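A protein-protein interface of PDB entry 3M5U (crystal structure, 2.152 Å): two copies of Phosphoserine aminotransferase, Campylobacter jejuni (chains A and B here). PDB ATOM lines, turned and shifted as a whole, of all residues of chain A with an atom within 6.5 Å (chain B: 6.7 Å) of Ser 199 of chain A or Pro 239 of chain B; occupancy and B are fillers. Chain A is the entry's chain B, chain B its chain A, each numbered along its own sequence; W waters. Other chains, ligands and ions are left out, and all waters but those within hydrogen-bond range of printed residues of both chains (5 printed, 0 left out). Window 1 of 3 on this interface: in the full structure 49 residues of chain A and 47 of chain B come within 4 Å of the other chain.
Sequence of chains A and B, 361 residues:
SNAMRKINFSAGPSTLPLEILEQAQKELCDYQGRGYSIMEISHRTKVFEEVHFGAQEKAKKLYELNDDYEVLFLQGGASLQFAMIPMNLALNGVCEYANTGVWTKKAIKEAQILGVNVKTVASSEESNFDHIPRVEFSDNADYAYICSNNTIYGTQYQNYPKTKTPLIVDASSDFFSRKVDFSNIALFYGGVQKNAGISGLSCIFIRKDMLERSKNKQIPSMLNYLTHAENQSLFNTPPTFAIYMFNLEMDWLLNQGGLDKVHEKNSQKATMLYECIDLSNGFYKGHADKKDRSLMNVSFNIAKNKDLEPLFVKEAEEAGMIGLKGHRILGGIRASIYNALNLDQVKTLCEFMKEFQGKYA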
ATOM      1  N   PRO A  13      17.493  15.320  -1.391  1.00  0.00           N
ATOM      2  CA  PRO A  13      16.499  15.772  -2.376  1.00  0.00           C
ATOM      3  C   PRO A  13      15.071  15.421  -1.956  1.00  0.00           C
ATOM      4  O   PRO A  13      14.857  14.531  -1.155  1.00  0.00           O
ATOM      5  CB  PRO A  13      16.897  15.052  -3.673  1.00  0.00           C
ATOM      6  CG  PRO A  13      18.352  14.771  -3.515  1.00  0.00           C
ATOM      7  CD  PRO A  13      18.596  14.572  -2.024  1.00  0.00           C
ATOM      8  N   VAL A 192      19.009  23.911  -4.588  1.00  0.00           N
ATOM      9  CA  VAL A 192      17.734  24.040  -5.262  1.00  0.00           C
ATOM     10  C   VAL A 192      16.796  22.856  -4.910  1.00  0.00           C
ATOM     11  O   VAL A 192      15.558  22.982  -4.973  1.00  0.00           O
ATOM     12  CB  VAL A 192      17.993  24.115  -6.785  1.00  0.00           C
ATOM     13  CG1 VAL A 192      17.049  23.199  -7.588  1.00  0.00           C
ATOM     14  CG2 VAL A 192      18.085  25.568  -7.275  1.00  0.00           C
ATOM     15  N   GLN A 193      17.396  21.725  -4.531  1.00  0.00           N
ATOM     16  CA  GLN A 193      16.665  20.460  -4.342  1.00  0.00           C
ATOM     17  C   GLN A 193      15.784  20.343  -3.078  1.00  0.00           C
ATOM     18  O   GLN A 193      15.290  19.257  -2.770  1.00  0.00           O
ATOM     19  CB  GLN A 193      17.645  19.303  -4.330  1.00  0.00           C
ATOM     20  CG  GLN A 193      18.463  19.232  -3.047  1.00  0.00           C
ATOM     21  CD  GLN A 193      19.610  20.247  -3.004  1.00  0.00           C
ATOM     22  OE1 GLN A 193      19.569  21.274  -3.681  1.00  0.00           O
ATOM     23  NE2 GLN A 193      20.645  19.952  -2.197  1.00  0.00           N
ATOM     24  N   GLY A 197      13.493  22.191  -7.273  1.00  0.00           N
ATOM     25  CA  GLY A 197      13.913  21.246  -8.278  1.00  0.00           C
ATOM     26  C   GLY A 197      14.893  20.190  -7.811  1.00  0.00           C
ATOM     27  O   GLY A 197      14.659  19.500  -6.798  1.00  0.00           O
ATOM     28  N   ILE A 198      15.985  20.029  -8.560  1.00  0.00           N
ATOM     29  CA  ILE A 198      16.858  18.887  -8.313  1.00  0.00           C
ATOM     30  C   ILE A 198      18.260  19.263  -7.854  1.00  0.00           C
ATOM     31  O   ILE A 198      18.666  20.429  -7.947  1.00  0.00           O
ATOM     32  CB  ILE A 198      16.887  17.902  -9.514  1.00  0.00           C
ATOM     33  CG1 ILE A 198      17.774  18.423 -10.652  1.00  0.00           C
ATOM     34  CG2 ILE A 198      15.462  17.621  -9.990  1.00  0.00           C
ATOM     35  CD1 ILE A 198      18.373  17.278 -11.515  1.00  0.00           C
ATOM     36  N   SER A 199      18.980  18.271  -7.331  1.00  0.00           N
ATOM     37  CA  SER A 199      20.276  18.528  -6.724  1.00  0.00           C
ATOM     38  C   SER A 199      21.293  18.844  -7.806  1.00  0.00           C
ATOM     39  O   SER A 199      21.190  18.356  -8.921  1.00  0.00           O
ATOM     40  CB  SER A 199      20.758  17.333  -5.890  1.00  0.00           C
ATOM     41  OG  SER A 199      20.875  16.161  -6.674  1.00  0.00           O
ATOM     42  N   GLY A 200      22.286  19.646  -7.467  1.00  0.00           N
ATOM     43  CA  GLY A 200      23.365  19.889  -8.412  1.00  0.00           C
ATOM     44  C   GLY A 200      23.279  21.299  -8.941  1.00  0.00           C
ATOM     45  O   GLY A 200      24.104  21.729  -9.745  1.00  0.00           O
ATOM     46  N   LEU A 201      22.272  22.034  -8.470  1.00  0.00           N
ATOM     47  CA  LEU A 201      22.085  23.393  -8.917  1.00  0.00           C
ATOM     48  C   LEU A 201      21.861  24.247  -7.697  1.00  0.00           C
ATOM     49  O   LEU A 201      21.141  23.847  -6.788  1.00  0.00           O
ATOM     50  CB  LEU A 201      20.888  23.468  -9.860  1.00  0.00           C
ATOM     51  CG  LEU A 201      20.524  24.886 -10.321  1.00  0.00           C
ATOM     52  CD1 LEU A 201      21.728  25.591 -11.019  1.00  0.00           C
ATOM     53  CD2 LEU A 201      19.276  24.873 -11.212  1.00  0.00           C
ATOM     54  N   PRO A 239      24.572  23.040 -15.258  1.00  0.00           N
ATOM     55  CA  PRO A 239      23.889  21.740 -15.288  1.00  0.00           C
ATOM     56  C   PRO A 239      22.580  21.913 -16.049  1.00  0.00           C
ATOM     57  O   PRO A 239      21.606  22.433 -15.502  1.00  0.00           O
ATOM     58  CB  PRO A 239      23.662  21.425 -13.800  1.00  0.00           C
ATOM     59  CG  PRO A 239      23.641  22.770 -13.128  1.00  0.00           C
ATOM     60  CD  PRO A 239      24.542  23.676 -13.929  1.00  0.00           C
ATOM     61  N   ALA A 242      19.207  20.235 -14.731  1.00  0.00           N
ATOM     62  CA  ALA A 242      18.794  20.892 -13.491  1.00  0.00           C
ATOM     63  C   ALA A 242      18.151  22.271 -13.738  1.00  0.00           C
ATOM     64  O   ALA A 242      17.150  22.612 -13.099  1.00  0.00           O
ATOM     65  CB  ALA A 242      19.974  21.001 -12.493  1.00  0.00           C
ATOM     66  N   MET B  39      15.379  10.796  -8.913  1.00  0.00           N
ATOM     67  CA  MET B  39      15.680  12.196  -8.678  1.00  0.00           C
ATOM     68  C   MET B  39      15.206  12.689  -7.338  1.00  0.00           C
ATOM     69  O   MET B  39      15.460  13.822  -6.981  1.00  0.00           O
ATOM     70  CB  MET B  39      14.955  13.032  -9.712  1.00  0.00           C
ATOM     71  CG  MET B  39      15.812  13.578 -10.784  1.00  0.00           C
ATOM     72  SD  MET B  39      14.706  14.328 -12.125  1.00  0.00           S
ATOM     73  CE  MET B  39      13.979  12.695 -12.808  1.00  0.00           C
ATOM     74  N   PHE B  48      20.162   4.625  -3.273  1.00  0.00           N
ATOM     75  CA  PHE B  48      21.110   5.490  -3.976  1.00  0.00           C
ATOM     76  C   PHE B  48      22.543   5.002  -3.875  1.00  0.00           C
ATOM     77  O   PHE B  48      23.323   5.123  -4.830  1.00  0.00           O
ATOM     78  CB  PHE B  48      21.069   6.966  -3.549  1.00  0.00           C
ATOM     79  CG  PHE B  48      22.085   7.799  -4.287  1.00  0.00           C
ATOM     80  CD1 PHE B  48      21.843   8.199  -5.606  1.00  0.00           C
ATOM     81  CD2 PHE B  48      23.327   8.084  -3.715  1.00  0.00           C
ATOM     82  CE1 PHE B  48      22.814   8.928  -6.328  1.00  0.00           C
ATOM     83  CE2 PHE B  48      24.300   8.796  -4.430  1.00  0.00           C
ATOM     84  CZ  PHE B  48      24.030   9.227  -5.737  1.00  0.00           C
ATOM     85  N   PHE B  73      33.115  11.439  -7.396  1.00  0.00           N
ATOM     86  CA  PHE B  73      32.054  12.053  -8.200  1.00  0.00           C
ATOM     87  C   PHE B  73      31.840  13.452  -7.639  1.00  0.00           C
ATOM     88  O   PHE B  73      31.417  13.576  -6.507  1.00  0.00           O
ATOM     89  CB  PHE B  73      30.770  11.217  -8.107  1.00  0.00           C
ATOM     90  CG  PHE B  73      30.876   9.858  -8.774  1.00  0.00           C
ATOM     91  CD1 PHE B  73      31.539   9.714  -9.988  1.00  0.00           C
ATOM     92  CD2 PHE B  73      30.279   8.742  -8.218  1.00  0.00           C
ATOM     93  CE1 PHE B  73      31.639   8.470 -10.626  1.00  0.00           C
ATOM     94  CE2 PHE B  73      30.384   7.478  -8.855  1.00  0.00           C
ATOM     95  CZ  PHE B  73      31.072   7.353 -10.050  1.00  0.00           C
ATOM     96  N   LEU B  74      32.234  14.486  -8.386  1.00  0.00           N
ATOM     97  CA  LEU B  74      32.110  15.870  -7.927  1.00  0.00           C
ATOM     98  C   LEU B  74      31.232  16.688  -8.883  1.00  0.00           C
ATOM     99  O   LEU B  74      30.946  16.261 -10.001  1.00  0.00           O
ATOM    100  CB  LEU B  74      33.482  16.548  -7.802  1.00  0.00           C
ATOM    101  CG  LEU B  74      34.617  15.796  -7.102  1.00  0.00           C
ATOM    102  CD1 LEU B  74      35.928  16.592  -7.117  1.00  0.00           C
ATOM    103  CD2 LEU B  74      34.245  15.431  -5.689  1.00  0.00           C
ATOM    104  N   GLN B  75      30.821  17.870  -8.434  1.00  0.00           N
ATOM    105  CA  GLN B  75      30.099  18.834  -9.272  1.00  0.00           C
ATOM    106  C   GLN B  75      31.060  19.906  -9.780  1.00  0.00           C
ATOM    107  O   GLN B  75      32.187  20.039  -9.259  1.00  0.00           O
ATOM    108  CB  GLN B  75      29.042  19.505  -8.443  1.00  0.00           C
ATOM    109  CG  GLN B  75      28.106  18.539  -7.718  1.00  0.00           C
ATOM    110  CD  GLN B  75      26.911  19.266  -7.085  1.00  0.00           C
ATOM    111  OE1 GLN B  75      26.520  20.357  -7.531  1.00  0.00           O
ATOM    112  NE2 GLN B  75      26.317  18.656  -6.055  1.00  0.00           N
ATOM    113  N   GLY B  76      30.631  20.661 -10.798  1.00  0.00           N
ATOM    114  CA  GLY B  76      31.357  21.846 -11.231  1.00  0.00           C
ATOM    115  C   GLY B  76      32.117  21.676 -12.545  1.00  0.00           C
ATOM    116  O   GLY B  76      32.893  22.557 -12.970  1.00  0.00           O
ATOM    117  N   SER B 199      25.785  16.782 -17.950  1.00  0.00           N
ATOM    118  CA  SER B 199      26.620  17.802 -17.322  1.00  0.00           C
ATOM    119  C   SER B 199      26.316  17.981 -15.844  1.00  0.00           C
ATOM    120  O   SER B 199      25.242  17.599 -15.356  1.00  0.00           O
ATOM    121  CB  SER B 199      26.547  19.134 -18.070  1.00  0.00           C
ATOM    122  OG  SER B 199      25.222  19.419 -18.447  1.00  0.00           O
ATOM    123  N   GLY B 200      27.279  18.551 -15.127  1.00  0.00           N
ATOM    124  CA  GLY B 200      27.100  18.822 -13.713  1.00  0.00           C
ATOM    125  C   GLY B 200      27.805  17.798 -12.840  1.00  0.00           C
ATOM    126  O   GLY B 200      27.861  17.931 -11.619  1.00  0.00           O
ATOM    127  N   LEU B 201      28.346  16.776 -13.484  1.00  0.00           N
ATOM    128  CA  LEU B 201      29.090  15.730 -12.816  1.00  0.00           C
ATOM    129  C   LEU B 201      30.467  15.580 -13.458  1.00  0.00           C
ATOM    130  O   LEU B 201      30.586  15.553 -14.683  1.00  0.00           O
ATOM    131  CB  LEU B 201      28.358  14.407 -12.991  1.00  0.00           C
ATOM    132  CG  LEU B 201      29.095  13.235 -12.367  1.00  0.00           C
ATOM    133  CD1 LEU B 201      29.198  13.439 -10.843  1.00  0.00           C
ATOM    134  CD2 LEU B 201      28.367  11.945 -12.745  1.00  0.00           C
ATOM    135  N   SER B 202      31.496  15.488 -12.630  1.00  0.00           N
ATOM    136  CA  SER B 202      32.822  15.175 -13.102  1.00  0.00           C
ATOM    137  C   SER B 202      33.273  13.865 -12.433  1.00  0.00           C
ATOM    138  O   SER B 202      32.920  13.571 -11.285  1.00  0.00           O
ATOM    139  CB  SER B 202      33.789  16.329 -12.825  1.00  0.00           C
ATOM    140  OG  SER B 202      34.060  16.422 -11.430  1.00  0.00           O
ATOM    141  N   SER B 233      32.612  10.626  -1.778  1.00  0.00           N
ATOM    142  CA  SER B 233      31.824  11.521  -2.654  1.00  0.00           C
ATOM    143  C   SER B 233      30.350  11.768  -2.199  1.00  0.00           C
ATOM    144  O   SER B 233      29.446  12.023  -3.027  1.00  0.00           O
ATOM    145  CB  SER B 233      31.898  11.043  -4.109  1.00  0.00           C
ATOM    146  OG  SER B 233      33.227  11.176  -4.574  1.00  0.00           O
ATOM    147  N   THR B 237      25.346  16.809  -0.719  1.00  0.00           N
ATOM    148  CA  THR B 237      24.486  16.138  -1.700  1.00  0.00           C
ATOM    149  C   THR B 237      25.238  16.026  -3.029  1.00  0.00           C
ATOM    150  O   THR B 237      25.706  17.048  -3.542  1.00  0.00           O
ATOM    151  CB  THR B 237      23.137  16.918  -1.934  1.00  0.00           C
ATOM    152  OG1 THR B 237      22.584  17.363  -0.680  1.00  0.00           O
ATOM    153  CG2 THR B 237      22.111  16.043  -2.677  1.00  0.00           C
ATOM    154  N   PRO B 238      25.368  14.798  -3.589  1.00  0.00           N
ATOM    155  CA  PRO B 238      25.943  14.681  -4.947  1.00  0.00           C
ATOM    156  C   PRO B 238      24.851  14.887  -6.007  1.00  0.00           C
ATOM    157  O   PRO B 238      23.663  15.022  -5.662  1.00  0.00           O
ATOM    158  CB  PRO B 238      26.421  13.232  -4.993  1.00  0.00           C
ATOM    159  CG  PRO B 238      25.306  12.487  -4.219  1.00  0.00           C
ATOM    160  CD  PRO B 238      24.919  13.486  -3.073  1.00  0.00           C
ATOM    161  N   PRO B 239      25.231  14.923  -7.292  1.00  0.00           N
ATOM    162  CA  PRO B 239      24.159  15.118  -8.276  1.00  0.00           C
ATOM    163  C   PRO B 239      23.564  13.750  -8.545  1.00  0.00           C
ATOM    164  O   PRO B 239      24.007  13.023  -9.425  1.00  0.00           O
ATOM    165  CB  PRO B 239      24.894  15.679  -9.510  1.00  0.00           C
ATOM    166  CG  PRO B 239      26.358  15.864  -9.072  1.00  0.00           C
ATOM    167  CD  PRO B 239      26.565  14.938  -7.910  1.00  0.00           C
ATOM    168  N   THR B 240      22.580  13.390  -7.740  1.00  0.00           N
ATOM    169  CA  THR B 240      22.089  12.030  -7.695  1.00  0.00           C
ATOM    170  C   THR B 240      21.687  11.545  -9.087  1.00  0.00           C
ATOM    171  O   THR B 240      22.089  10.476  -9.506  1.00  0.00           O
ATOM    172  CB  THR B 240      20.899  11.930  -6.750  1.00  0.00           C
ATOM    173  OG1 THR B 240      19.933  12.938  -7.096  1.00  0.00           O
ATOM    174  CG2 THR B 240      21.367  12.158  -5.328  1.00  0.00           C
ATOM    175  N   PHE B 241      20.897  12.340  -9.795  1.00  0.00           N
ATOM    176  CA  PHE B 241      20.428  11.937 -11.107  1.00  0.00           C
ATOM    177  C   PHE B 241      21.591  11.663 -12.082  1.00  0.00           C
ATOM    178  O   PHE B 241      21.641  10.617 -12.751  1.00  0.00           O
ATOM    179  CB  PHE B 241      19.470  12.981 -11.688  1.00  0.00           C
ATOM    180  CG  PHE B 241      18.805  12.509 -12.931  1.00  0.00           C
ATOM    181  CD1 PHE B 241      17.975  11.410 -12.893  1.00  0.00           C
ATOM    182  CD2 PHE B 241      19.031  13.133 -14.137  1.00  0.00           C
ATOM    183  CE1 PHE B 241      17.361  10.956 -14.046  1.00  0.00           C
ATOM    184  CE2 PHE B 241      18.415  12.692 -15.276  1.00  0.00           C
ATOM    185  CZ  PHE B 241      17.597  11.583 -15.236  1.00  0.00           C
ATOM    186  N   ALA B 242      22.511  12.626 -12.160  1.00  0.00           N
ATOM    187  CA  ALA B 242      23.745  12.517 -12.933  1.00  0.00           C
ATOM    188  C   ALA B 242      24.522  11.216 -12.663  1.00  0.00           C
ATOM    189  O   ALA B 242      24.979  10.538 -13.594  1.00  0.00           O
ATOM    190  CB  ALA B 242      24.644  13.755 -12.682  1.00  0.00           C
ATOM    191  N   ILE B 243      24.658  10.873 -11.392  1.00  0.00           N
ATOM    192  CA  ILE B 243      25.329   9.650 -11.000  1.00  0.00           C
ATOM    193  C   ILE B 243      24.518   8.438 -11.451  1.00  0.00           C
ATOM    194  O   ILE B 243      25.069   7.416 -11.882  1.00  0.00           O
ATOM    195  CB  ILE B 243      25.613   9.640  -9.478  1.00  0.00           C
ATOM    196  CG1 ILE B 243      26.700  10.678  -9.171  1.00  0.00           C
ATOM    197  CG2 ILE B 243      26.007   8.265  -9.016  1.00  0.00           C
ATOM    198  CD1 ILE B 243      27.080  10.815  -7.728  1.00  0.00           C
ATOM    199  N   TYR B 244      23.201   8.562 -11.378  1.00  0.00           N
ATOM    200  CA  TYR B 244      22.342   7.490 -11.845  1.00  0.00           C
ATOM    201  C   TYR B 244      22.506   7.248 -13.346  1.00  0.00           C
ATOM    202  O   TYR B 244      22.509   6.106 -13.767  1.00  0.00           O
ATOM    203  CB  TYR B 244      20.901   7.804 -11.525  1.00  0.00           C
ATOM    204  CG  TYR B 244      19.874   7.168 -12.450  1.00  0.00           C
ATOM    205  CD1 TYR B 244      19.334   5.924 -12.158  1.00  0.00           C
ATOM    206  CD2 TYR B 244      19.420   7.838 -13.612  1.00  0.00           C
ATOM    207  CE1 TYR B 244      18.363   5.327 -12.987  1.00  0.00           C
ATOM    208  CE2 TYR B 244      18.458   7.261 -14.437  1.00  0.00           C
ATOM    209  CZ  TYR B 244      17.917   6.006 -14.102  1.00  0.00           C
ATOM    210  OH  TYR B 244      16.947   5.408 -14.890  1.00  0.00           O
HETATM  211  O   HOH W   1      19.826  15.596  -9.298  1.00  0.00           O
HETATM  212  O   HOH W   2      24.646  22.812  -6.784  1.00  0.00           O
HETATM  213  O   HOH W   3      17.854  15.305  -7.278  1.00  0.00           O
HETATM  214  O   HOH W   4      15.048  16.964  -5.649  1.00  0.00           O
HETATM  215  O   HOH W   5      20.095  17.739   0.157  1.00  0.00           O
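OG of Ser 199 of chain A sits at hydrogen-bond distance from OG1 of Thr 240 of chain B, at 3.4 Å. O of Pro 238 of chain B is in hydrogen-bond range of OG of Ser 199 of chain A (3.2 Å).
The backbone carbonyl oxygen (O) of Thr 237 of chain B is in hydrogen-bond range of the side-chain amide nitrogen (NE2) of Gln 75 of chain B (3.0 Å).
Among the printed residues, pairs that only touch across the chains: Gly 200 of chain A with Gln 75 of chain B (3.3 Å), Gln 193 of chain A with Thr 237 of chain B (3.6 Å), Ser 199 of chain A with Thr 237 of chain B (3.7 Å), Ser 199 of chain A with Pro 239 of chain B (3.8 Å), Pro 13 of chain A with Met 39 of chain B (3.8 Å), Pro 13 of chain A with Thr 237 of chain B (3.9 Å) and Ile 198 of chain A with Met 39 of chain B (3.997 Å).
Of the printed residues of chain A, Pro 239 of chain B touches Ser 199. Of the printed residues of chain B, Gln 193 of chain A touches Thr 237. Of the printed residues of chain B, Gly 200 of chain A touches Gln 75. Printed residues of chain B within 4 Å of Ile 198 of chain A: Met 39 (3.997 Å). Of the printed residues of chain A, Met 39 of chain B touches Pro 13 (3.8 Å) and Ile 198 (3.997 Å). Tyr 244 of chain B touches none of the printed residues of chain A. The nearest residue of chain B that does not touch Ser 199 of chain A is Phe 241 of chain B (4.9 Å). The nearest printed residue of chain A that does not touch Thr 237 of chain B is Gly 200 of chain A (5.8 Å).
Hydrophobic or aromatic side chains of chain A that line the printed part of chain B: Pro 13 and Ile 198. Hydrophobic or aromatic side chains of chain B that line the printed part of chain A: Met 39. Among the printed residues, no Asp or Glu carboxylate lies within 4 Å of a Lys or Arg side-chain nitrogen of the other chain.
Ser 199 of chain A touches Pro 239 of chain B, but with the chains exchanged Pro 239 of chain A does not touch Ser 199 of chain B (4.1 Å). Of the 9 pairs that touch across the chains among the printed residues, none has its exchanged pair printed and touching as well.
Water W5 lies within hydrogen-bond range of OG1 of Thr 237 of chain B and NE2 of Gln 193 of chain A. Water W4 lies within hydrogen-bond range of O of Gly 197 of chain A and O of Met 39 of chain B. Water W3 lies within hydrogen-bond range of O of Met 39 of chain B, OG1 of Thr 240 of chain B and N of Ser 199 of chain A. Water W1 lies within hydrogen-bond range of the side-chain hydroxyl of Ser 199 of chain A (2.9 Å), the side-chain hydroxyl of Thr 240 of chain B (3.5 Å) and the backbone NH of Phe 241 of chain B (3.5 Å). Water W2 lies within hydrogen-bond range of the backbone NH of Leu 201 of chain A (3.0 Å), the side-chain amide oxygen of Gln 75 of chain B (3.2 Å) and the backbone carbonyl oxygen of Gly 200 of chain A (3.2 Å).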
